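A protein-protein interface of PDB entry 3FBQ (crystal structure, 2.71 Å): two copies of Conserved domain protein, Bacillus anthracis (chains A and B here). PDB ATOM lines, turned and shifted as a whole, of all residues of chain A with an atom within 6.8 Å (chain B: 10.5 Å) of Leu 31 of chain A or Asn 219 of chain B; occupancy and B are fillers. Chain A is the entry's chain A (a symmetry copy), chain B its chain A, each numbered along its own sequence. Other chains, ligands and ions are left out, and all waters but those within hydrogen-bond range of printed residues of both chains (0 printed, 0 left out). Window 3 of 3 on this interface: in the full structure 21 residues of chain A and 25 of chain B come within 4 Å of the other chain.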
ATOM      1  N   THR A  29      30.672  -7.984  17.324  1.00  0.00           N
ATOM      2  CA  THR A  29      29.410  -8.678  17.486  1.00  0.00           C
ATOM      3  C   THR A  29      28.986  -8.353  18.886  1.00  0.00           C
ATOM      4  O   THR A  29      29.709  -8.658  19.887  1.00  0.00           O
ATOM      5  CB  THR A  29      29.569 -10.195  17.428  1.00  0.00           C
ATOM      6  OG1 THR A  29      30.314 -10.553  16.272  1.00  0.00           O
ATOM      7  CG2 THR A  29      28.230 -10.889  17.473  1.00  0.00           C
ATOM      8  N   GLU A  30      27.824  -7.736  18.938  1.00  0.00           N
ATOM      9  CA  GLU A  30      27.290  -7.255  20.169  1.00  0.00           C
ATOM     10  C   GLU A  30      26.567  -8.408  20.796  1.00  0.00           C
ATOM     11  O   GLU A  30      25.717  -8.987  20.125  1.00  0.00           O
ATOM     12  CB  GLU A  30      26.290  -6.140  19.890  1.00  0.00           C
ATOM     13  CG  GLU A  30      25.199  -6.054  20.913  1.00  0.00           C
ATOM     14  CD  GLU A  30      24.555  -4.676  20.932  1.00  0.00           C
ATOM     15  OE1 GLU A  30      25.214  -3.740  21.432  1.00  0.00           O
ATOM     16  OE2 GLU A  30      23.398  -4.535  20.421  1.00  0.00           O
ATOM     17  N   LEU A  31      26.875  -8.759  22.049  1.00  0.00           N
ATOM     18  CA  LEU A  31      26.010  -9.754  22.630  1.00  0.00           C
ATOM     19  C   LEU A  31      25.294  -9.490  23.942  1.00  0.00           C
ATOM     20  O   LEU A  31      24.217 -10.005  24.163  1.00  0.00           O
ATOM     21  CB  LEU A  31      26.544 -11.167  22.474  1.00  0.00           C
ATOM     22  CG  LEU A  31      27.922 -11.712  22.788  1.00  0.00           C
ATOM     23  CD1 LEU A  31      27.894 -12.254  24.185  1.00  0.00           C
ATOM     24  CD2 LEU A  31      28.057 -12.842  21.836  1.00  0.00           C
ATOM     25  N   ASN A  32      25.824  -8.650  24.795  1.00  0.00           N
ATOM     26  CA  ASN A  32      25.069  -8.320  25.974  1.00  0.00           C
ATOM     27  C   ASN A  32      24.484  -9.587  26.632  1.00  0.00           C
ATOM     28  O   ASN A  32      23.423  -9.596  27.187  1.00  0.00           O
ATOM     29  CB  ASN A  32      24.024  -7.242  25.678  1.00  0.00           C
ATOM     30  CG  ASN A  32      24.622  -6.023  25.034  1.00  0.00           C
ATOM     31  OD1 ASN A  32      25.688  -5.532  25.436  1.00  0.00           O
ATOM     32  ND2 ASN A  32      23.968  -5.536  23.985  1.00  0.00           N
ATOM     33  N   MET A  33      25.214 -10.679  26.572  1.00  0.00           N
ATOM     34  CA  MET A  33      24.830 -11.883  27.318  1.00  0.00           C
ATOM     35  C   MET A  33      25.264 -11.800  28.821  1.00  0.00           C
ATOM     36  O   MET A  33      26.401 -11.414  29.130  1.00  0.00           O
ATOM     37  CB  MET A  33      25.300 -13.098  26.536  1.00  0.00           C
ATOM     38  CG  MET A  33      26.033 -14.138  27.277  1.00  0.00           C
ATOM     39  SD  MET A  33      26.442 -15.439  26.047  1.00  0.00           S
ATOM     40  CE  MET A  33      25.094 -16.633  26.358  1.00  0.00           C
ATOM     41  N   THR A  34      24.329 -12.082  29.727  1.00  0.00           N
ATOM     42  CA  THR A  34      24.517 -11.835  31.167  1.00  0.00           C
ATOM     43  C   THR A  34      24.574 -13.092  32.037  1.00  0.00           C
ATOM     44  O   THR A  34      23.896 -14.055  31.756  1.00  0.00           O
ATOM     45  CB  THR A  34      23.377 -10.958  31.744  1.00  0.00           C
ATOM     46  OG1 THR A  34      23.133  -9.876  30.843  1.00  0.00           O
ATOM     47  CG2 THR A  34      23.779 -10.356  33.032  1.00  0.00           C
ATOM     48  N   ARG A  35      25.394 -13.030  33.084  1.00  0.00           N
ATOM     49  CA  ARG A  35      25.467 -13.990  34.167  1.00  0.00           C
ATOM     50  C   ARG A  35      25.337 -13.302  35.516  1.00  0.00           C
ATOM     51  O   ARG A  35      25.967 -12.281  35.750  1.00  0.00           O
ATOM     52  CB  ARG A  35      26.802 -14.736  34.124  1.00  0.00           C
ATOM     53  CG  ARG A  35      26.687 -16.177  33.600  1.00  0.00           C
ATOM     54  CD  ARG A  35      25.758 -16.225  32.417  1.00  0.00           C
ATOM     55  NE  ARG A  35      26.251 -17.088  31.362  1.00  0.00           N
ATOM     56  CZ  ARG A  35      25.775 -17.125  30.123  1.00  0.00           C
ATOM     57  NH1 ARG A  35      24.783 -16.321  29.727  1.00  0.00           N
ATOM     58  NH2 ARG A  35      26.313 -17.985  29.283  1.00  0.00           N
ATOM     59  N   THR A  43      28.137  -8.874  32.412  1.00  0.00           N
ATOM     60  CA  THR A  43      27.730  -8.854  31.029  1.00  0.00           C
ATOM     61  C   THR A  43      28.928  -8.833  30.134  1.00  0.00           C
ATOM     62  O   THR A  43      29.905  -8.140  30.404  1.00  0.00           O
ATOM     63  CB  THR A  43      26.968  -7.608  30.750  1.00  0.00           C
ATOM     64  OG1 THR A  43      25.883  -7.631  31.656  1.00  0.00           O
ATOM     65  CG2 THR A  43      26.359  -7.573  29.276  1.00  0.00           C
ATOM     66  N   ILE A  44      28.862  -9.599  29.050  1.00  0.00           N
ATOM     67  CA  ILE A  44      29.940  -9.632  28.068  1.00  0.00           C
ATOM     68  C   ILE A  44      29.505  -8.994  26.753  1.00  0.00           C
ATOM     69  O   ILE A  44      28.846  -9.631  25.930  1.00  0.00           O
ATOM     70  CB  ILE A  44      30.413 -11.073  27.798  1.00  0.00           C
ATOM     71  CG1 ILE A  44      31.775 -11.317  28.451  1.00  0.00           C
ATOM     72  CG2 ILE A  44      30.478 -11.339  26.303  1.00  0.00           C
ATOM     73  CD1 ILE A  44      32.700 -12.184  27.626  1.00  0.00           C
ATOM     74  N   ASN A  45      29.879  -7.734  26.560  1.00  0.00           N
ATOM     75  CA  ASN A  45      29.191  -6.867  25.610  1.00  0.00           C
ATOM     76  C   ASN A  45      29.638  -7.118  24.174  1.00  0.00           C
ATOM     77  O   ASN A  45      29.069  -7.957  23.475  1.00  0.00           O
ATOM     78  CB  ASN A  45      29.402  -5.397  25.978  1.00  0.00           C
ATOM     79  CG  ASN A  45      28.643  -4.993  27.226  1.00  0.00           C
ATOM     80  OD1 ASN A  45      27.416  -4.897  27.216  1.00  0.00           O
ATOM     81  ND2 ASN A  45      29.370  -4.755  28.311  1.00  0.00           N
ATOM     82  N   ASP A  46      30.658  -6.386  23.740  1.00  0.00           N
ATOM     83  CA  ASP A  46      31.154  -6.495  22.373  1.00  0.00           C
ATOM     84  C   ASP A  46      32.152  -7.640  22.239  1.00  0.00           C
ATOM     85  O   ASP A  46      32.947  -7.892  23.145  1.00  0.00           O
ATOM     86  CB  ASP A  46      31.798  -5.181  21.929  1.00  0.00           C
ATOM     87  CG  ASP A  46      30.778  -4.086  21.682  1.00  0.00           C
ATOM     88  OD1 ASP A  46      31.187  -2.963  21.318  1.00  0.00           O
ATOM     89  OD2 ASP A  46      29.569  -4.349  21.851  1.00  0.00           O
ATOM     90  N   VAL A  47      32.105  -8.329  21.104  1.00  0.00           N
ATOM     91  CA  VAL A  47      33.014  -9.440  20.845  1.00  0.00           C
ATOM     92  C   VAL A  47      33.620  -9.343  19.448  1.00  0.00           C
ATOM     93  O   VAL A  47      32.948  -8.945  18.496  1.00  0.00           O
ATOM     94  CB  VAL A  47      32.302 -10.798  20.992  1.00  0.00           C
ATOM     95  CG1 VAL A  47      31.236 -10.957  19.918  1.00  0.00           C
ATOM     96  CG2 VAL A  47      33.310 -11.935  20.925  1.00  0.00           C
ATOM     97  N   PHE A 117      36.026 -19.958  23.047  1.00  0.00           N
ATOM     98  CA  PHE A 117      36.694 -19.574  24.298  1.00  0.00           C
ATOM     99  C   PHE A 117      35.809 -19.776  25.516  1.00  0.00           C
ATOM    100  O   PHE A 117      34.607 -19.954  25.331  1.00  0.00           O
ATOM    101  CB  PHE A 117      37.186 -18.149  24.190  1.00  0.00           C
ATOM    102  CG  PHE A 117      36.092 -17.197  24.040  1.00  0.00           C
ATOM    103  CD1 PHE A 117      35.547 -16.591  25.152  1.00  0.00           C
ATOM    104  CD2 PHE A 117      35.521 -16.966  22.770  1.00  0.00           C
ATOM    105  CE1 PHE A 117      34.493 -15.694  25.028  1.00  0.00           C
ATOM    106  CE2 PHE A 117      34.440 -16.050  22.610  1.00  0.00           C
ATOM    107  CZ  PHE A 117      33.944 -15.398  23.747  1.00  0.00           C
ATOM    108  N   PHE A 139      31.016 -17.901  30.827  1.00  0.00           N
ATOM    109  CA  PHE A 139      30.496 -17.863  29.475  1.00  0.00           C
ATOM    110  C   PHE A 139      31.356 -18.792  28.671  1.00  0.00           C
ATOM    111  O   PHE A 139      32.591 -18.754  28.757  1.00  0.00           O
ATOM    112  CB  PHE A 139      30.515 -16.452  28.862  1.00  0.00           C
ATOM    113  CG  PHE A 139      29.988 -15.349  29.776  1.00  0.00           C
ATOM    114  CD1 PHE A 139      28.825 -14.685  29.472  1.00  0.00           C
ATOM    115  CD2 PHE A 139      30.681 -14.968  30.930  1.00  0.00           C
ATOM    116  CE1 PHE A 139      28.334 -13.651  30.318  1.00  0.00           C
ATOM    117  CE2 PHE A 139      30.197 -13.972  31.788  1.00  0.00           C
ATOM    118  CZ  PHE A 139      29.036 -13.294  31.482  1.00  0.00           C
ATOM    119  N   LEU A 141      31.585 -19.724  24.652  1.00  0.00           N
ATOM    120  CA  LEU A 141      31.017 -19.422  23.339  1.00  0.00           C
ATOM    121  C   LEU A 141      32.062 -19.413  22.213  1.00  0.00           C
ATOM    122  O   LEU A 141      33.253 -19.305  22.463  1.00  0.00           O
ATOM    123  CB  LEU A 141      30.163 -18.129  23.425  1.00  0.00           C
ATOM    124  CG  LEU A 141      30.812 -16.974  24.181  1.00  0.00           C
ATOM    125  CD1 LEU A 141      31.165 -16.006  23.153  1.00  0.00           C
ATOM    126  CD2 LEU A 141      29.883 -16.290  25.164  1.00  0.00           C
ATOM    127  N   ASN B 181      11.592 -17.074  34.978  1.00  0.00           N
ATOM    128  CA  ASN B 181      12.291 -16.059  34.155  1.00  0.00           C
ATOM    129  C   ASN B 181      11.524 -14.787  34.050  1.00  0.00           C
ATOM    130  O   ASN B 181      10.319 -14.797  34.223  1.00  0.00           O
ATOM    131  CB  ASN B 181      12.603 -16.542  32.742  1.00  0.00           C
ATOM    132  CG  ASN B 181      11.390 -16.991  32.011  1.00  0.00           C
ATOM    133  OD1 ASN B 181      10.448 -16.238  31.740  1.00  0.00           O
ATOM    134  ND2 ASN B 181      11.403 -18.246  31.674  1.00  0.00           N
ATOM    135  N   GLN B 182      12.243 -13.702  33.743  1.00  0.00           N
ATOM    136  CA  GLN B 182      11.672 -12.381  33.575  1.00  0.00           C
ATOM    137  C   GLN B 182      11.764 -12.110  32.113  1.00  0.00           C
ATOM    138  O   GLN B 182      12.728 -12.531  31.472  1.00  0.00           O
ATOM    139  CB  GLN B 182      12.448 -11.312  34.369  1.00  0.00           C
ATOM    140  CG  GLN B 182      13.958 -11.275  34.180  1.00  0.00           C
ATOM    141  CD  GLN B 182      14.656 -10.204  35.044  1.00  0.00           C
ATOM    142  OE1 GLN B 182      15.361  -9.295  34.531  1.00  0.00           O
ATOM    143  NE2 GLN B 182      14.497 -10.324  36.360  1.00  0.00           N
ATOM    144  N   ARG B 189      12.394  -1.699  28.524  1.00  0.00           N
ATOM    145  CA  ARG B 189      13.874  -1.766  28.424  1.00  0.00           C
ATOM    146  C   ARG B 189      14.450  -0.367  28.311  1.00  0.00           C
ATOM    147  O   ARG B 189      15.573  -0.091  28.776  1.00  0.00           O
ATOM    148  CB  ARG B 189      14.353  -2.558  27.200  1.00  0.00           C
ATOM    149  CG  ARG B 189      13.775  -3.924  27.062  1.00  0.00           C
ATOM    150  CD  ARG B 189      14.600  -4.739  26.133  1.00  0.00           C
ATOM    151  NE  ARG B 189      14.328  -6.132  26.391  1.00  0.00           N
ATOM    152  CZ  ARG B 189      15.129  -7.145  26.094  1.00  0.00           C
ATOM    153  NH1 ARG B 189      16.306  -6.944  25.503  1.00  0.00           N
ATOM    154  NH2 ARG B 189      14.747  -8.380  26.412  1.00  0.00           N
ATOM    155  N   GLY B 216      21.224 -16.387  37.802  1.00  0.00           N
ATOM    156  CA  GLY B 216      20.499 -16.161  36.561  1.00  0.00           C
ATOM    157  C   GLY B 216      21.382 -16.061  35.328  1.00  0.00           C
ATOM    158  O   GLY B 216      22.601 -15.870  35.410  1.00  0.00           O
ATOM    159  N   SER B 217      20.732 -16.153  34.174  1.00  0.00           N
ATOM    160  CA  SER B 217      21.338 -16.267  32.879  1.00  0.00           C
ATOM    161  C   SER B 217      20.413 -15.628  31.843  1.00  0.00           C
ATOM    162  O   SER B 217      19.192 -15.707  31.981  1.00  0.00           O
ATOM    163  CB  SER B 217      21.411 -17.729  32.529  1.00  0.00           C
ATOM    164  OG  SER B 217      22.608 -18.262  32.993  1.00  0.00           O
ATOM    165  N   GLY B 218      20.999 -15.076  30.778  1.00  0.00           N
ATOM    166  CA  GLY B 218      20.265 -14.452  29.700  1.00  0.00           C
ATOM    167  C   GLY B 218      21.189 -14.137  28.545  1.00  0.00           C
ATOM    168  O   GLY B 218      22.404 -14.014  28.724  1.00  0.00           O
ATOM    169  N   ASN B 219      20.605 -14.036  27.352  1.00  0.00           N
ATOM    170  CA  ASN B 219      21.322 -13.610  26.148  1.00  0.00           C
ATOM    171  C   ASN B 219      21.141 -12.148  25.904  1.00  0.00           C
ATOM    172  O   ASN B 219      21.769 -11.591  25.035  1.00  0.00           O
ATOM    173  CB  ASN B 219      20.863 -14.388  24.943  1.00  0.00           C
ATOM    174  CG  ASN B 219      20.998 -15.864  25.162  1.00  0.00           C
ATOM    175  OD1 ASN B 219      22.109 -16.418  25.095  1.00  0.00           O
ATOM    176  ND2 ASN B 219      19.887 -16.512  25.495  1.00  0.00           N
ATOM    177  N   ASP B 220      20.277 -11.520  26.670  1.00  0.00           N
ATOM    178  CA  ASP B 220      20.337 -10.106  26.741  1.00  0.00           C
ATOM    179  C   ASP B 220      20.297  -9.680  28.186  1.00  0.00           C
ATOM    180  O   ASP B 220      20.163 -10.517  29.071  1.00  0.00           O
ATOM    181  CB  ASP B 220      19.304  -9.434  25.834  1.00  0.00           C
ATOM    182  CG  ASP B 220      17.881  -9.734  26.211  1.00  0.00           C
ATOM    183  OD1 ASP B 220      17.196 -10.367  25.364  1.00  0.00           O
ATOM    184  OD2 ASP B 220      17.456  -9.328  27.321  1.00  0.00           O
ATOM    185  N   PRO B 221      20.491  -8.378  28.434  1.00  0.00           N
ATOM    186  CA  PRO B 221      20.630  -8.021  29.827  1.00  0.00           C
ATOM    187  C   PRO B 221      19.345  -8.115  30.636  1.00  0.00           C
ATOM    188  O   PRO B 221      19.413  -7.856  31.831  1.00  0.00           O
ATOM    189  CB  PRO B 221      21.138  -6.551  29.760  1.00  0.00           C
ATOM    190  CG  PRO B 221      21.805  -6.449  28.472  1.00  0.00           C
ATOM    191  CD  PRO B 221      21.016  -7.315  27.549  1.00  0.00           C
ATOM    192  N   TYR B 222      18.225  -8.521  30.012  1.00  0.00           N
ATOM    193  CA  TYR B 222      16.845  -8.312  30.539  1.00  0.00           C
ATOM    194  C   TYR B 222      16.032  -9.568  30.716  1.00  0.00           C
ATOM    195  O   TYR B 222      15.396  -9.739  31.758  1.00  0.00           O
ATOM    196  CB  TYR B 222      16.015  -7.468  29.581  1.00  0.00           C
ATOM    197  CG  TYR B 222      16.492  -6.072  29.416  1.00  0.00           C
ATOM    198  CD1 TYR B 222      17.302  -5.718  28.322  1.00  0.00           C
ATOM    199  CD2 TYR B 222      16.145  -5.084  30.348  1.00  0.00           C
ATOM    200  CE1 TYR B 222      17.751  -4.401  28.145  1.00  0.00           C
ATOM    201  CE2 TYR B 222      16.616  -3.753  30.195  1.00  0.00           C
ATOM    202  CZ  TYR B 222      17.413  -3.427  29.086  1.00  0.00           C
ATOM    203  OH  TYR B 222      17.867  -2.137  28.939  1.00  0.00           O
ATOM    204  N   ASN B 223      15.968 -10.394  29.667  1.00  0.00           N
ATOM    205  CA  ASN B 223      15.322 -11.704  29.750  1.00  0.00           C
ATOM    206  C   ASN B 223      16.223 -12.788  30.395  1.00  0.00           C
ATOM    207  O   ASN B 223      17.008 -13.460  29.685  1.00  0.00           O
ATOM    208  CB  ASN B 223      14.896 -12.133  28.355  1.00  0.00           C
ATOM    209  CG  ASN B 223      13.656 -11.362  27.847  1.00  0.00           C
ATOM    210  OD1 ASN B 223      13.422 -10.167  28.163  1.00  0.00           O
ATOM    211  ND2 ASN B 223      12.849 -12.057  27.053  1.00  0.00           N
ATOM    212  N   ILE B 224      16.110 -12.933  31.725  1.00  0.00           N
ATOM    213  CA  ILE B 224      16.970 -13.784  32.529  1.00  0.00           C
ATOM    214  C   ILE B 224      16.158 -14.995  33.065  1.00  0.00           C
ATOM    215  O   ILE B 224      15.161 -14.810  33.730  1.00  0.00           O
ATOM    216  CB  ILE B 224      17.611 -12.988  33.766  1.00  0.00           C
ATOM    217  CG1 ILE B 224      18.214 -11.610  33.412  1.00  0.00           C
ATOM    218  CG2 ILE B 224      18.607 -13.778  34.526  1.00  0.00           C
ATOM    219  CD1 ILE B 224      18.800 -11.509  32.079  1.00  0.00           C
ATOM    220  N   ARG B 225      16.601 -16.221  32.801  1.00  0.00           N
ATOM    221  CA  ARG B 225      16.143 -17.388  33.528  1.00  0.00           C
ATOM    222  C   ARG B 225      16.873 -17.402  34.845  1.00  0.00           C
ATOM    223  O   ARG B 225      18.083 -17.137  34.877  1.00  0.00           O
ATOM    224  CB  ARG B 225      16.447 -18.659  32.757  1.00  0.00           C
ATOM    225  CG  ARG B 225      16.247 -18.450  31.226  1.00  0.00           C
ATOM    226  CD  ARG B 225      16.141 -19.744  30.456  1.00  0.00           C
ATOM    227  NE  ARG B 225      15.420 -20.764  31.238  1.00  0.00           N
ATOM    228  CZ  ARG B 225      15.470 -22.077  30.989  1.00  0.00           C
ATOM    229  NH1 ARG B 225      16.213 -22.524  29.975  1.00  0.00           N
ATOM    230  NH2 ARG B 225      14.798 -22.949  31.754  1.00  0.00           N
ATOM    231  N   TRP B 226      16.131 -17.695  35.926  1.00  0.00           N
ATOM    232  CA  TRP B 226      16.634 -17.687  37.294  1.00  0.00           C
ATOM    233  C   TRP B 226      16.154 -18.934  37.961  1.00  0.00           C
ATOM    234  O   TRP B 226      15.231 -19.615  37.495  1.00  0.00           O
ATOM    235  CB  TRP B 226      15.932 -16.596  38.113  1.00  0.00           C
ATOM    236  CG  TRP B 226      16.030 -15.207  37.700  1.00  0.00           C
ATOM    237  CD1 TRP B 226      15.089 -14.485  37.004  1.00  0.00           C
ATOM    238  CD2 TRP B 226      17.058 -14.317  38.023  1.00  0.00           C
ATOM    239  NE1 TRP B 226      15.510 -13.190  36.836  1.00  0.00           N
ATOM    240  CE2 TRP B 226      16.734 -13.070  37.444  1.00  0.00           C
ATOM    241  CE3 TRP B 226      18.274 -14.453  38.703  1.00  0.00           C
ATOM    242  CZ2 TRP B 226      17.584 -11.964  37.535  1.00  0.00           C
ATOM    243  CZ3 TRP B 226      19.133 -13.361  38.790  1.00  0.00           C
ATOM    244  CH2 TRP B 226      18.790 -12.137  38.209  1.00  0.00           C
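The backbone carbonyl oxygen (O) of Gly 218 of chain B sits at hydrogen-bond distance from the backbone NH (N) of Thr 34 of chain A (2.9 Å).
The backbone carbonyl oxygen of Gly 218 of chain B lies within hydrogen-bond range of the guanidinium group of Arg 35 of chain A, at 3.5 Å.
O of Asn 219 of chain B lies close to O of Asn 32 of chain A (3.4 Å).
O of Asn 219 of chain B lies close to O of Leu 31 of chain A, at 3.0 Å.
The backbone nitrogen (N) of Pro 221 of chain B sits close to the backbone carbonyl oxygen (O) of Asn 32 of chain A.
No position is printed for both chains.
Of the 14 printed residues of chain B, 6 touch a printed residue of chain A.
Printed residues of chain B that touch a printed residue of chain A: Gly 216, Ser 217, Gly 218, Asn 219, Asp 220 and Pro 221.
Hydrophobic or aromatic side chains of chain B within 4 Å of the printed part of chain A: Pro 221.
Among the printed residues, 13 pairs touch across the chains.
Asp 220 of chain B touches Asn 32 of chain A.
Gly 218 of chain B touches Met 33 of chain A.
OD1 of Asn 219 of chain B touches CE of Met 33 of chain A, 3.2 Å away.
Ser 217 of chain B touches Thr 34 of chain A.
Thr 34 of chain A touches Asp 220 of chain B.
Pro 221 of chain B touches Thr 34 of chain A (CA to OG1, 3.3 Å).
Arg 35 of chain A touches Gly 216 of chain B (CA to O, 3.6 Å).
Ser 217 of chain B touches Arg 35 of chain A (OG to CD, 3.8 Å).
The backbone carbonyl oxygen (O) of Ile 44 of chain A lies within hydrogen-bond range of the backbone NH (N) of Asn 32 of chain A (3.4 Å).
The side-chain amide nitrogen (ND2) of Asn 32 of chain A sits close to the side-chain carboxylate (OE1) of Glu 30 of chain A, 3.4 Å away.
OD2 of Asp 220 of chain B lies within hydrogen-bond range of N of Asn 223 of chain B (3.0 Å).
OD1 of Asn 32 of chain A sits close to OD1 of Asn 45 of chain A (2.6 Å).
N of Leu 31 of chain A lies within hydrogen-bond range of O of Asn 45 of chain A (2.7 Å).
The backbone NH of Ile 44 of chain A is in hydrogen-bond range of the backbone carbonyl oxygen of Met 33 of chain A, at 3.1 Å.
No residue of chain B comes within 4 Å of Thr 29 of chain A.
No residue of chain B comes within 4 Å of Glu 30 of chain A.
Leu 31 of chain A touches just one residue of chain B: Asn 219 (3.0 Å).
No residue of chain B comes within 4 Å of Ile 44 of chain A.
Of the printed residues of chain A, Gly 216 of chain B touches Arg 35 (3.6 Å).
Asn 219 of chain B touches three residues of chain A.
Printed residues of chain A within 4 Å of Asp 220 of chain B: Asn 32 and Thr 34.
Of the printed residues of chain A, Pro 221 of chain B touches Asn 32 and Thr 34.
The nearest residue of chain A that does not touch Asn 219 of chain B is Thr 34 of chain A (4.8 Å).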
